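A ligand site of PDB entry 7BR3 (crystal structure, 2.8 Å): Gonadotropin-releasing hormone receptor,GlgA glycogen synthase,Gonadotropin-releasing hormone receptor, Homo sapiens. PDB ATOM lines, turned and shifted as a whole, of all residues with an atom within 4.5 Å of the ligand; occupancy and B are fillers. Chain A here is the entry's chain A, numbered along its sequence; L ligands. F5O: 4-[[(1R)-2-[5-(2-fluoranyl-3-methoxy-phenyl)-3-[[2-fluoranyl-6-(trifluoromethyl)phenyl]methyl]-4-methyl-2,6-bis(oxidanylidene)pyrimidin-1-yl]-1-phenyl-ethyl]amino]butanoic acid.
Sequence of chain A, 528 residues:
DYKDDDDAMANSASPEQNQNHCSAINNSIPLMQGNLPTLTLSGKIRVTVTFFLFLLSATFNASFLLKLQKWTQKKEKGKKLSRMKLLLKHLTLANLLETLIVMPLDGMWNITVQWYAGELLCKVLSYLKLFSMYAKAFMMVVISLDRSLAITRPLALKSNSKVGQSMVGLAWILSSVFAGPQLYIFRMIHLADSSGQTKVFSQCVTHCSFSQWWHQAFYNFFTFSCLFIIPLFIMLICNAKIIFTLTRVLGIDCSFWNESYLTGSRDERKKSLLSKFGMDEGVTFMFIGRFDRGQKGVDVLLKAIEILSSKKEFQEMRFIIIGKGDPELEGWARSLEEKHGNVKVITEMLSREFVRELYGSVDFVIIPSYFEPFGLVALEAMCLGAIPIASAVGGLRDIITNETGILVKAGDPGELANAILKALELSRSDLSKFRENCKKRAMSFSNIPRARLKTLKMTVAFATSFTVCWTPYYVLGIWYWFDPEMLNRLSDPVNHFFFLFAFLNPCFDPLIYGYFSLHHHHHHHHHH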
ATOM      1  N   ILE A  29      34.063 -29.322 -31.239  1.00  0.00           N
ATOM      2  CA  ILE A  29      33.311 -28.203 -30.686  1.00  0.00           C
ATOM      3  C   ILE A  29      32.996 -27.188 -31.781  1.00  0.00           C
ATOM      4  O   ILE A  29      33.910 -26.589 -32.346  1.00  0.00           O
ATOM      5  CB  ILE A  29      34.058 -27.509 -29.536  1.00  0.00           C
ATOM      6  CG1 ILE A  29      34.195 -28.440 -28.329  1.00  0.00           C
ATOM      7  CG2 ILE A  29      33.367 -26.200 -29.164  1.00  0.00           C
ATOM      8  CD1 ILE A  29      34.936 -27.826 -27.161  1.00  0.00           C
ATOM      9  N   PRO A  30      31.716 -26.936 -32.088  1.00  0.00           N
ATOM     10  CA  PRO A  30      31.399 -25.953 -33.139  1.00  0.00           C
ATOM     11  C   PRO A  30      31.643 -24.516 -32.706  1.00  0.00           C
ATOM     12  O   PRO A  30      30.702 -23.758 -32.468  1.00  0.00           O
ATOM     13  CB  PRO A  30      29.910 -26.204 -33.414  1.00  0.00           C
ATOM     14  CG  PRO A  30      29.385 -26.771 -32.138  1.00  0.00           C
ATOM     15  CD  PRO A  30      30.515 -27.583 -31.546  1.00  0.00           C
ATOM     16  N   LEU A  31      32.921 -24.132 -32.619  1.00  0.00           N
ATOM     17  CA  LEU A  31      33.254 -22.766 -32.201  1.00  0.00           C
ATOM     18  C   LEU A  31      32.986 -21.730 -33.292  1.00  0.00           C
ATOM     19  O   LEU A  31      32.792 -20.552 -32.979  1.00  0.00           O
ATOM     20  CB  LEU A  31      34.717 -22.710 -31.769  1.00  0.00           C
ATOM     21  CG  LEU A  31      35.091 -21.516 -30.901  1.00  0.00           C
ATOM     22  CD1 LEU A  31      34.917 -21.877 -29.448  1.00  0.00           C
ATOM     23  CD2 LEU A  31      36.525 -21.082 -31.178  1.00  0.00           C
ATOM     24  N   MET A  32      32.986 -22.144 -34.552  1.00  0.00           N
ATOM     25  CA  MET A  32      32.793 -21.221 -35.657  1.00  0.00           C
ATOM     26  C   MET A  32      31.712 -21.737 -36.605  1.00  0.00           C
ATOM     27  O   MET A  32      31.782 -21.547 -37.819  1.00  0.00           O
ATOM     28  CB  MET A  32      34.100 -21.009 -36.413  1.00  0.00           C
ATOM     29  CG  MET A  32      35.180 -20.298 -35.611  1.00  0.00           C
ATOM     30  SD  MET A  32      34.807 -18.563 -35.292  1.00  0.00           S
ATOM     31  CE  MET A  32      34.800 -17.870 -36.941  1.00  0.00           C
ATOM     32  N   GLN A  33      30.683 -22.374 -36.059  1.00  0.00           N
ATOM     33  CA  GLN A  33      29.635 -22.963 -36.885  1.00  0.00           C
ATOM     34  C   GLN A  33      28.321 -23.029 -36.117  1.00  0.00           C
ATOM     35  O   GLN A  33      28.265 -23.633 -35.043  1.00  0.00           O
ATOM     36  CB  GLN A  33      30.041 -24.352 -37.348  1.00  0.00           C
ATOM     37  CG  GLN A  33      29.011 -25.017 -38.225  1.00  0.00           C
ATOM     38  CD  GLN A  33      29.452 -26.386 -38.678  1.00  0.00           C
ATOM     39  OE1 GLN A  33      29.997 -27.157 -37.884  1.00  0.00           O
ATOM     40  NE2 GLN A  33      29.240 -26.686 -39.954  1.00  0.00           N
ATOM     41  N   GLY A  34      27.272 -22.449 -36.701  1.00  0.00           N
ATOM     42  CA  GLY A  34      25.956 -22.462 -36.092  1.00  0.00           C
ATOM     43  C   GLY A  34      25.232 -23.791 -36.272  1.00  0.00           C
ATOM     44  O   GLY A  34      25.709 -24.706 -36.924  1.00  0.00           O
ATOM     45  N   ASN A  35      24.042 -23.872 -35.681  1.00  0.00           N
ATOM     46  CA  ASN A  35      23.301 -25.136 -35.631  1.00  0.00           C
ATOM     47  C   ASN A  35      21.877 -24.992 -36.134  1.00  0.00           C
ATOM     48  O   ASN A  35      20.973 -25.720 -35.696  1.00  0.00           O
ATOM     49  CB  ASN A  35      23.318 -25.715 -34.215  1.00  0.00           C
ATOM     50  CG  ASN A  35      24.484 -26.651 -33.991  1.00  0.00           C
ATOM     51  OD1 ASN A  35      25.368 -26.368 -33.173  1.00  0.00           O
ATOM     52  ND2 ASN A  35      24.504 -27.766 -34.711  1.00  0.00           N
ATOM     53  N   ASP A 106      28.637 -14.611 -33.335  1.00  0.00           N
ATOM     54  CA  ASP A 106      27.834 -15.735 -32.836  1.00  0.00           C
ATOM     55  C   ASP A 106      26.338 -15.438 -32.771  1.00  0.00           C
ATOM     56  O   ASP A 106      25.535 -16.373 -32.681  1.00  0.00           O
ATOM     57  CB  ASP A 106      28.325 -16.148 -31.455  1.00  0.00           C
ATOM     58  CG  ASP A 106      29.570 -17.005 -31.518  1.00  0.00           C
ATOM     59  OD1 ASP A 106      30.002 -17.321 -32.649  1.00  0.00           O
ATOM     60  OD2 ASP A 106      30.120 -17.358 -30.453  1.00  0.00           O
ATOM     61  N   ASN A 110      26.978 -15.553 -38.294  1.00  0.00           N
ATOM     62  CA  ASN A 110      27.298 -16.969 -38.444  1.00  0.00           C
ATOM     63  C   ASN A 110      26.453 -17.849 -37.514  1.00  0.00           C
ATOM     64  O   ASN A 110      26.956 -18.553 -36.636  1.00  0.00           O
ATOM     65  CB  ASN A 110      28.794 -17.195 -38.207  1.00  0.00           C
ATOM     66  CG  ASN A 110      29.227 -18.620 -38.522  1.00  0.00           C
ATOM     67  OD1 ASN A 110      28.743 -19.246 -39.476  1.00  0.00           O
ATOM     68  ND2 ASN A 110      30.147 -19.147 -37.721  1.00  0.00           N
ATOM     69  N   ILE A 111      25.145 -17.813 -37.727  1.00  0.00           N
ATOM     70  CA  ILE A 111      24.197 -18.537 -36.896  1.00  0.00           C
ATOM     71  C   ILE A 111      23.618 -19.773 -37.585  1.00  0.00           C
ATOM     72  O   ILE A 111      23.115 -20.669 -36.879  1.00  0.00           O
ATOM     73  CB  ILE A 111      23.059 -17.619 -36.411  1.00  0.00           C
ATOM     74  CG1 ILE A 111      22.379 -16.927 -37.587  1.00  0.00           C
ATOM     75  CG2 ILE A 111      23.587 -16.571 -35.433  1.00  0.00           C
ATOM     76  CD1 ILE A 111      21.031 -16.342 -37.235  1.00  0.00           C
ATOM     77  N   LYS A 129      37.826 -14.147 -32.095  1.00  0.00           N
ATOM     78  CA  LYS A 129      36.841 -14.634 -31.138  1.00  0.00           C
ATOM     79  C   LYS A 129      37.516 -15.077 -29.848  1.00  0.00           C
ATOM     80  O   LYS A 129      37.197 -14.589 -28.764  1.00  0.00           O
ATOM     81  CB  LYS A 129      36.022 -15.774 -31.731  1.00  0.00           C
ATOM     82  CG  LYS A 129      35.118 -16.437 -30.692  1.00  0.00           C
ATOM     83  CD  LYS A 129      34.234 -17.528 -31.287  1.00  0.00           C
ATOM     84  CE  LYS A 129      33.276 -18.066 -30.239  1.00  0.00           C
ATOM     85  NZ  LYS A 129      32.409 -19.136 -30.776  1.00  0.00           N
ATOM     86  N   MET A 133      37.935 -13.091 -25.855  1.00  0.00           N
ATOM     87  CA  MET A 133      37.432 -13.738 -24.658  1.00  0.00           C
ATOM     88  C   MET A 133      38.551 -14.075 -23.688  1.00  0.00           C
ATOM     89  O   MET A 133      38.377 -13.935 -22.475  1.00  0.00           O
ATOM     90  CB  MET A 133      36.653 -14.996 -25.047  1.00  0.00           C
ATOM     91  CG  MET A 133      35.521 -14.693 -25.996  1.00  0.00           C
ATOM     92  SD  MET A 133      34.702 -16.181 -26.598  1.00  0.00           S
ATOM     93  CE  MET A 133      33.638 -16.543 -25.215  1.00  0.00           C
ATOM     94  N   ASN A 220      40.948 -28.437 -26.546  1.00  0.00           N
ATOM     95  CA  ASN A 220      39.689 -27.902 -26.047  1.00  0.00           C
ATOM     96  C   ASN A 220      39.676 -27.833 -24.527  1.00  0.00           C
ATOM     97  O   ASN A 220      39.056 -26.937 -23.954  1.00  0.00           O
ATOM     98  CB  ASN A 220      38.515 -28.717 -26.561  1.00  0.00           C
ATOM     99  CG  ASN A 220      38.365 -28.603 -28.052  1.00  0.00           C
ATOM    100  OD1 ASN A 220      37.812 -27.624 -28.567  1.00  0.00           O
ATOM    101  ND2 ASN A 220      38.839 -29.615 -28.770  1.00  0.00           N
ATOM    102  N   THR A 223      41.507 -24.726 -23.843  1.00  0.00           N
ATOM    103  CA  THR A 223      40.661 -23.571 -24.115  1.00  0.00           C
ATOM    104  C   THR A 223      39.729 -23.288 -22.945  1.00  0.00           C
ATOM    105  O   THR A 223      39.579 -22.130 -22.534  1.00  0.00           O
ATOM    106  CB  THR A 223      39.868 -23.778 -25.404  1.00  0.00           C
ATOM    107  OG1 THR A 223      40.782 -23.993 -26.487  1.00  0.00           O
ATOM    108  CG2 THR A 223      39.024 -22.549 -25.701  1.00  0.00           C
ATOM    109  N   PHE A 224      39.108 -24.334 -22.380  1.00  0.00           N
ATOM    110  CA  PHE A 224      38.096 -24.116 -21.344  1.00  0.00           C
ATOM    111  C   PHE A 224      38.715 -23.577 -20.057  1.00  0.00           C
ATOM    112  O   PHE A 224      38.221 -22.609 -19.474  1.00  0.00           O
ATOM    113  CB  PHE A 224      37.359 -25.419 -21.078  1.00  0.00           C
ATOM    114  CG  PHE A 224      36.129 -25.596 -21.919  1.00  0.00           C
ATOM    115  CD1 PHE A 224      35.223 -24.563 -22.055  1.00  0.00           C
ATOM    116  CD2 PHE A 224      35.897 -26.797 -22.570  1.00  0.00           C
ATOM    117  CE1 PHE A 224      34.088 -24.726 -22.836  1.00  0.00           C
ATOM    118  CE2 PHE A 224      34.766 -26.970 -23.343  1.00  0.00           C
ATOM    119  CZ  PHE A 224      33.863 -25.931 -23.473  1.00  0.00           C
ATOM    120  N   LEU A 227      40.017 -20.099 -20.265  1.00  0.00           N
ATOM    121  CA  LEU A 227      38.973 -19.153 -20.634  1.00  0.00           C
ATOM    122  C   LEU A 227      38.029 -18.837 -19.488  1.00  0.00           C
ATOM    123  O   LEU A 227      37.413 -17.769 -19.509  1.00  0.00           O
ATOM    124  CB  LEU A 227      38.131 -19.697 -21.796  1.00  0.00           C
ATOM    125  CG  LEU A 227      37.864 -18.826 -23.020  1.00  0.00           C
ATOM    126  CD1 LEU A 227      39.132 -18.204 -23.554  1.00  0.00           C
ATOM    127  CD2 LEU A 227      37.218 -19.701 -24.078  1.00  0.00           C
ATOM    128  N   TYR A 473      26.723 -20.181 -19.599  1.00  0.00           N
ATOM    129  CA  TYR A 473      27.235 -20.270 -20.969  1.00  0.00           C
ATOM    130  C   TYR A 473      28.284 -21.362 -21.091  1.00  0.00           C
ATOM    131  O   TYR A 473      28.225 -22.192 -22.007  1.00  0.00           O
ATOM    132  CB  TYR A 473      27.808 -18.905 -21.393  1.00  0.00           C
ATOM    133  CG  TYR A 473      28.183 -18.775 -22.847  1.00  0.00           C
ATOM    134  CD1 TYR A 473      27.220 -18.592 -23.827  1.00  0.00           C
ATOM    135  CD2 TYR A 473      29.516 -18.801 -23.245  1.00  0.00           C
ATOM    136  CE1 TYR A 473      27.574 -18.466 -25.156  1.00  0.00           C
ATOM    137  CE2 TYR A 473      29.879 -18.681 -24.572  1.00  0.00           C
ATOM    138  CZ  TYR A 473      28.902 -18.514 -25.531  1.00  0.00           C
ATOM    139  OH  TYR A 473      29.243 -18.390 -26.854  1.00  0.00           O
ATOM    140  N   TYR A 474      29.244 -21.409 -20.161  1.00  0.00           N
ATOM    141  CA  TYR A 474      30.414 -22.269 -20.290  1.00  0.00           C
ATOM    142  C   TYR A 474      30.192 -23.708 -19.830  1.00  0.00           C
ATOM    143  O   TYR A 474      30.904 -24.604 -20.300  1.00  0.00           O
ATOM    144  CB  TYR A 474      31.591 -21.692 -19.505  1.00  0.00           C
ATOM    145  CG  TYR A 474      32.415 -20.694 -20.280  1.00  0.00           C
ATOM    146  CD1 TYR A 474      32.920 -20.995 -21.525  1.00  0.00           C
ATOM    147  CD2 TYR A 474      32.714 -19.449 -19.737  1.00  0.00           C
ATOM    148  CE1 TYR A 474      33.686 -20.094 -22.229  1.00  0.00           C
ATOM    149  CE2 TYR A 474      33.474 -18.537 -20.436  1.00  0.00           C
ATOM    150  CZ  TYR A 474      33.951 -18.862 -21.676  1.00  0.00           C
ATOM    151  OH  TYR A 474      34.712 -17.967 -22.373  1.00  0.00           O
ATOM    152  N   LEU A 476      27.325 -25.441 -20.256  1.00  0.00           N
ATOM    153  CA  LEU A 476      26.742 -26.054 -21.449  1.00  0.00           C
ATOM    154  C   LEU A 476      27.819 -26.303 -22.498  1.00  0.00           C
ATOM    155  O   LEU A 476      27.719 -27.260 -23.269  1.00  0.00           O
ATOM    156  CB  LEU A 476      25.639 -25.176 -22.027  1.00  0.00           C
ATOM    157  CG  LEU A 476      24.620 -24.546 -21.064  1.00  0.00           C
ATOM    158  CD1 LEU A 476      23.899 -23.403 -21.756  1.00  0.00           C
ATOM    159  CD2 LEU A 476      23.631 -25.589 -20.562  1.00  0.00           C
ATOM    160  N   GLY A 477      28.859 -25.465 -22.513  1.00  0.00           N
ATOM    161  CA  GLY A 477      30.003 -25.750 -23.359  1.00  0.00           C
ATOM    162  C   GLY A 477      30.702 -27.040 -22.975  1.00  0.00           C
ATOM    163  O   GLY A 477      30.981 -27.881 -23.824  1.00  0.00           O
ATOM    164  N   TYR A 480      28.250 -29.933 -23.527  1.00  0.00           N
ATOM    165  CA  TYR A 480      28.310 -30.340 -24.930  1.00  0.00           C
ATOM    166  C   TYR A 480      29.552 -31.191 -25.193  1.00  0.00           C
ATOM    167  O   TYR A 480      29.479 -32.217 -25.872  1.00  0.00           O
ATOM    168  CB  TYR A 480      28.302 -29.110 -25.839  1.00  0.00           C
ATOM    169  CG  TYR A 480      28.352 -29.468 -27.296  1.00  0.00           C
ATOM    170  CD1 TYR A 480      27.193 -29.766 -28.001  1.00  0.00           C
ATOM    171  CD2 TYR A 480      29.563 -29.548 -27.975  1.00  0.00           C
ATOM    172  CE1 TYR A 480      27.226 -30.125 -29.339  1.00  0.00           C
ATOM    173  CE2 TYR A 480      29.613 -29.916 -29.311  1.00  0.00           C
ATOM    174  CZ  TYR A 480      28.441 -30.190 -29.990  1.00  0.00           C
ATOM    175  OH  TYR A 480      28.470 -30.554 -31.321  1.00  0.00           O
ATOM    176  N   MET A 486      23.395 -33.503 -26.548  1.00  0.00           N
ATOM    177  CA  MET A 486      22.633 -32.733 -25.536  1.00  0.00           C
ATOM    178  C   MET A 486      21.975 -31.546 -26.223  1.00  0.00           C
ATOM    179  O   MET A 486      21.000 -31.028 -25.712  1.00  0.00           O
ATOM    180  CB  MET A 486      23.577 -32.183 -24.477  1.00  0.00           C
ATOM    181  CG  MET A 486      23.136 -30.840 -23.972  1.00  0.00           C
ATOM    182  SD  MET A 486      24.359 -29.541 -24.013  1.00  0.00           S
ATOM    183  CE  MET A 486      24.228 -28.897 -25.666  1.00  0.00           C
ATOM    184  N   LEU A 487      22.553 -31.122 -27.336  1.00  0.00           N
ATOM    185  CA  LEU A 487      22.046 -29.927 -28.063  1.00  0.00           C
ATOM    186  C   LEU A 487      20.639 -30.217 -28.576  1.00  0.00           C
ATOM    187  O   LEU A 487      19.854 -29.284 -28.658  1.00  0.00           O
ATOM    188  CB  LEU A 487      23.019 -29.638 -29.203  1.00  0.00           C
ATOM    189  CG  LEU A 487      22.998 -28.198 -29.704  1.00  0.00           C
ATOM    190  CD1 LEU A 487      23.125 -27.238 -28.538  1.00  0.00           C
ATOM    191  CD2 LEU A 487      24.110 -27.972 -30.689  1.00  0.00           C
ATOM    192  N   VAL A 494      15.915 -20.858 -25.092  1.00  0.00           N
ATOM    193  CA  VAL A 494      16.853 -20.953 -23.970  1.00  0.00           C
ATOM    194  C   VAL A 494      18.299 -20.890 -24.438  1.00  0.00           C
ATOM    195  O   VAL A 494      19.162 -20.343 -23.737  1.00  0.00           O
ATOM    196  CB  VAL A 494      16.585 -22.220 -23.111  1.00  0.00           C
ATOM    197  CG1 VAL A 494      15.109 -22.339 -22.750  1.00  0.00           C
ATOM    198  CG2 VAL A 494      17.100 -23.483 -23.790  1.00  0.00           C
ATOM    199  N   ASN A 495      18.591 -21.460 -25.607  1.00  0.00           N
ATOM    200  CA  ASN A 495      19.904 -21.221 -26.207  1.00  0.00           C
ATOM    201  C   ASN A 495      20.122 -19.725 -26.407  1.00  0.00           C
ATOM    202  O   ASN A 495      21.185 -19.188 -26.060  1.00  0.00           O
ATOM    203  CB  ASN A 495      20.039 -21.966 -27.533  1.00  0.00           C
ATOM    204  CG  ASN A 495      21.496 -22.117 -28.010  1.00  0.00           C
ATOM    205  OD1 ASN A 495      22.096 -23.193 -27.906  1.00  0.00           O
ATOM    206  ND2 ASN A 495      22.066 -21.024 -28.512  1.00  0.00           N
ATOM    207  N   PHE A 498      20.460 -17.960 -22.717  1.00  0.00           N
ATOM    208  CA  PHE A 498      21.758 -18.062 -22.060  1.00  0.00           C
ATOM    209  C   PHE A 498      22.865 -17.420 -22.869  1.00  0.00           C
ATOM    210  O   PHE A 498      23.924 -17.108 -22.318  1.00  0.00           O
ATOM    211  CB  PHE A 498      22.054 -19.527 -21.762  1.00  0.00           C
ATOM    212  CG  PHE A 498      21.242 -20.074 -20.626  1.00  0.00           C
ATOM    213  CD1 PHE A 498      21.240 -19.442 -19.392  1.00  0.00           C
ATOM    214  CD2 PHE A 498      20.459 -21.209 -20.787  1.00  0.00           C
ATOM    215  CE1 PHE A 498      20.475 -19.933 -18.339  1.00  0.00           C
ATOM    216  CE2 PHE A 498      19.700 -21.711 -19.740  1.00  0.00           C
ATOM    217  CZ  PHE A 498      19.717 -21.067 -18.512  1.00  0.00           C
ATOM    218  N   PHE A 499      22.665 -17.187 -24.165  1.00  0.00           N
ATOM    219  CA  PHE A 499      23.583 -16.338 -24.914  1.00  0.00           C
ATOM    220  C   PHE A 499      23.485 -14.890 -24.448  1.00  0.00           C
ATOM    221  O   PHE A 499      24.502 -14.240 -24.199  1.00  0.00           O
ATOM    222  CB  PHE A 499      23.316 -16.451 -26.406  1.00  0.00           C
ATOM    223  CG  PHE A 499      24.258 -15.641 -27.242  1.00  0.00           C
ATOM    224  CD1 PHE A 499      25.518 -16.129 -27.559  1.00  0.00           C
ATOM    225  CD2 PHE A 499      23.890 -14.394 -27.722  1.00  0.00           C
ATOM    226  CE1 PHE A 499      26.400 -15.382 -28.327  1.00  0.00           C
ATOM    227  CE2 PHE A 499      24.771 -13.647 -28.491  1.00  0.00           C
ATOM    228  CZ  PHE A 499      26.023 -14.147 -28.794  1.00  0.00           C
HETATM  229  CAA F5O L   1      26.164 -20.209 -33.100  1.00  0.00           C
HETATM  230  CAB F5O L   1      27.376 -19.330 -33.461  1.00  0.00           C
HETATM  231  CAC F5O L   1      28.636 -20.132 -33.888  1.00  0.00           C
HETATM  232  CAD F5O L   1      29.365 -20.797 -32.687  1.00  0.00           C
HETATM  233  CAH F5O L   1      28.909 -21.949 -30.702  1.00  0.00           C
HETATM  234  CAI F5O L   1      28.459 -20.771 -29.776  1.00  0.00           C
HETATM  235  CAJ F5O L   1      28.406 -23.266 -30.152  1.00  0.00           C
HETATM  236  CAK F5O L   1      27.055 -23.588 -30.207  1.00  0.00           C
HETATM  237  CAL F5O L   1      26.603 -24.812 -29.692  1.00  0.00           C
HETATM  238  CAM F5O L   1      27.507 -25.708 -29.128  1.00  0.00           C
HETATM  239  CAN F5O L   1      28.858 -25.386 -29.073  1.00  0.00           C
HETATM  240  CAO F5O L   1      29.302 -24.175 -29.588  1.00  0.00           C
HETATM  241  CAP F5O L   1      28.021 -21.383 -27.412  1.00  0.00           C
HETATM  242  CAR F5O L   1      29.695 -21.779 -25.870  1.00  0.00           C
HETATM  243  CAS F5O L   1      30.655 -21.509 -26.846  1.00  0.00           C
HETATM  244  CAT F5O L   1      30.212 -21.185 -28.124  1.00  0.00           C
HETATM  245  CAX F5O L   1      30.141 -22.157 -24.445  1.00  0.00           C
HETATM  246  CAY F5O L   1      27.387 -21.964 -25.121  1.00  0.00           C
HETATM  247  CAZ F5O L   1      26.367 -23.051 -25.411  1.00  0.00           C
HETATM  248  CBA F5O L   1      26.841 -24.309 -25.781  1.00  0.00           C
HETATM  249  CBB F5O L   1      25.955 -25.345 -26.044  1.00  0.00           C
HETATM  250  CBC F5O L   1      24.584 -25.126 -25.946  1.00  0.00           C
HETATM  251  CBD F5O L   1      24.113 -23.862 -25.569  1.00  0.00           C
HETATM  252  CBE F5O L   1      24.995 -22.831 -25.299  1.00  0.00           C
HETATM  253  CBF F5O L   1      24.375 -21.434 -24.882  1.00  0.00           C
HETATM  254  CBK F5O L   1      32.165 -21.587 -26.565  1.00  0.00           C
HETATM  255  CBL F5O L   1      32.765 -22.863 -26.421  1.00  0.00           C
HETATM  256  CBM F5O L   1      34.141 -22.991 -26.167  1.00  0.00           C
HETATM  257  CBN F5O L   1      34.931 -21.860 -26.062  1.00  0.00           C
HETATM  258  CBO F5O L   1      34.327 -20.573 -26.215  1.00  0.00           C
HETATM  259  CBP F5O L   1      32.951 -20.445 -26.468  1.00  0.00           C
HETATM  260  CBR F5O L   1      36.110 -24.390 -25.856  1.00  0.00           C
HETATM  261  FBG F5O L   1      24.585 -20.512 -25.828  1.00  0.00           F
HETATM  262  FBH F5O L   1      23.021 -21.633 -24.723  1.00  0.00           F
HETATM  263  FBI F5O L   1      24.887 -20.978 -23.702  1.00  0.00           F
HETATM  264  FBJ F5O L   1      28.175 -24.489 -25.871  1.00  0.00           F
HETATM  265  FBS F5O L   1      31.975 -23.995 -26.526  1.00  0.00           F
HETATM  266  NAG F5O L   1      28.473 -21.744 -32.044  1.00  0.00           N
HETATM  267  NAQ F5O L   1      28.386 -21.709 -26.184  1.00  0.00           N
HETATM  268  NAU F5O L   1      28.915 -21.122 -28.380  1.00  0.00           N
HETATM  269  OAE F5O L   1      25.009 -19.761 -33.268  1.00  0.00           O
HETATM  270  OAF F5O L   1      26.316 -21.363 -32.613  1.00  0.00           O
HETATM  271  OAV F5O L   1      31.199 -20.914 -29.112  1.00  0.00           O
HETATM  272  OAW F5O L   1      26.850 -21.323 -27.660  1.00  0.00           O
HETATM  273  OBQ F5O L   1      34.687 -24.318 -26.026  1.00  0.00           O
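The side-chain amino group of Lys 129 sits at hydrogen-bond distance from an oxygen (OAV) of the ligand (2.7 Å). O of Pro 30 sits at hydrogen-bond distance from NAG of the ligand (3.0 Å).
NZ of Lys 129 is in salt-bridge range of OD2 of Asp 106 (2.9 Å). The side-chain amide nitrogen (ND2) of Asn 110 sits at hydrogen-bond distance from the backbone carbonyl oxygen (O) of Met 32. NZ of Lys 129 is in hydrogen-bond range of O of Leu 31 (2.6 Å).
OAE of the ligand sits close to O of Asp 106, 3.5 Å away. The side-chain hydroxyl (OH) of Tyr 473 sits close to a nitrogen (NAU) of the ligand (3.1 Å). O of Asn 495 sits close to FBH of the ligand. Residues that only touch the ligand: Phe 224 (3.1 Å), Leu 476 (3.3 Å), Asn 110 (3.3 Å), Gly 477 (3.4 Å), Leu 31 (3.4 Å), Thr 223 (3.5 Å), Gln 33 (3.6 Å), Leu 487 (3.6 Å), Gly 34 (3.7 Å), Ile 29 (3.7 Å), Leu 227 (3.7 Å), Phe 498 (3.7 Å), Met 486 (3.8 Å) and Ile 111 (3.9 Å). Hydrophobic or aromatic side chains within 4 Å of the ligand: Ile 29, Pro 30, Leu 31, Phe 224, Leu 227, Tyr 473, Leu 476, Met 486, Leu 487 and Phe 498.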
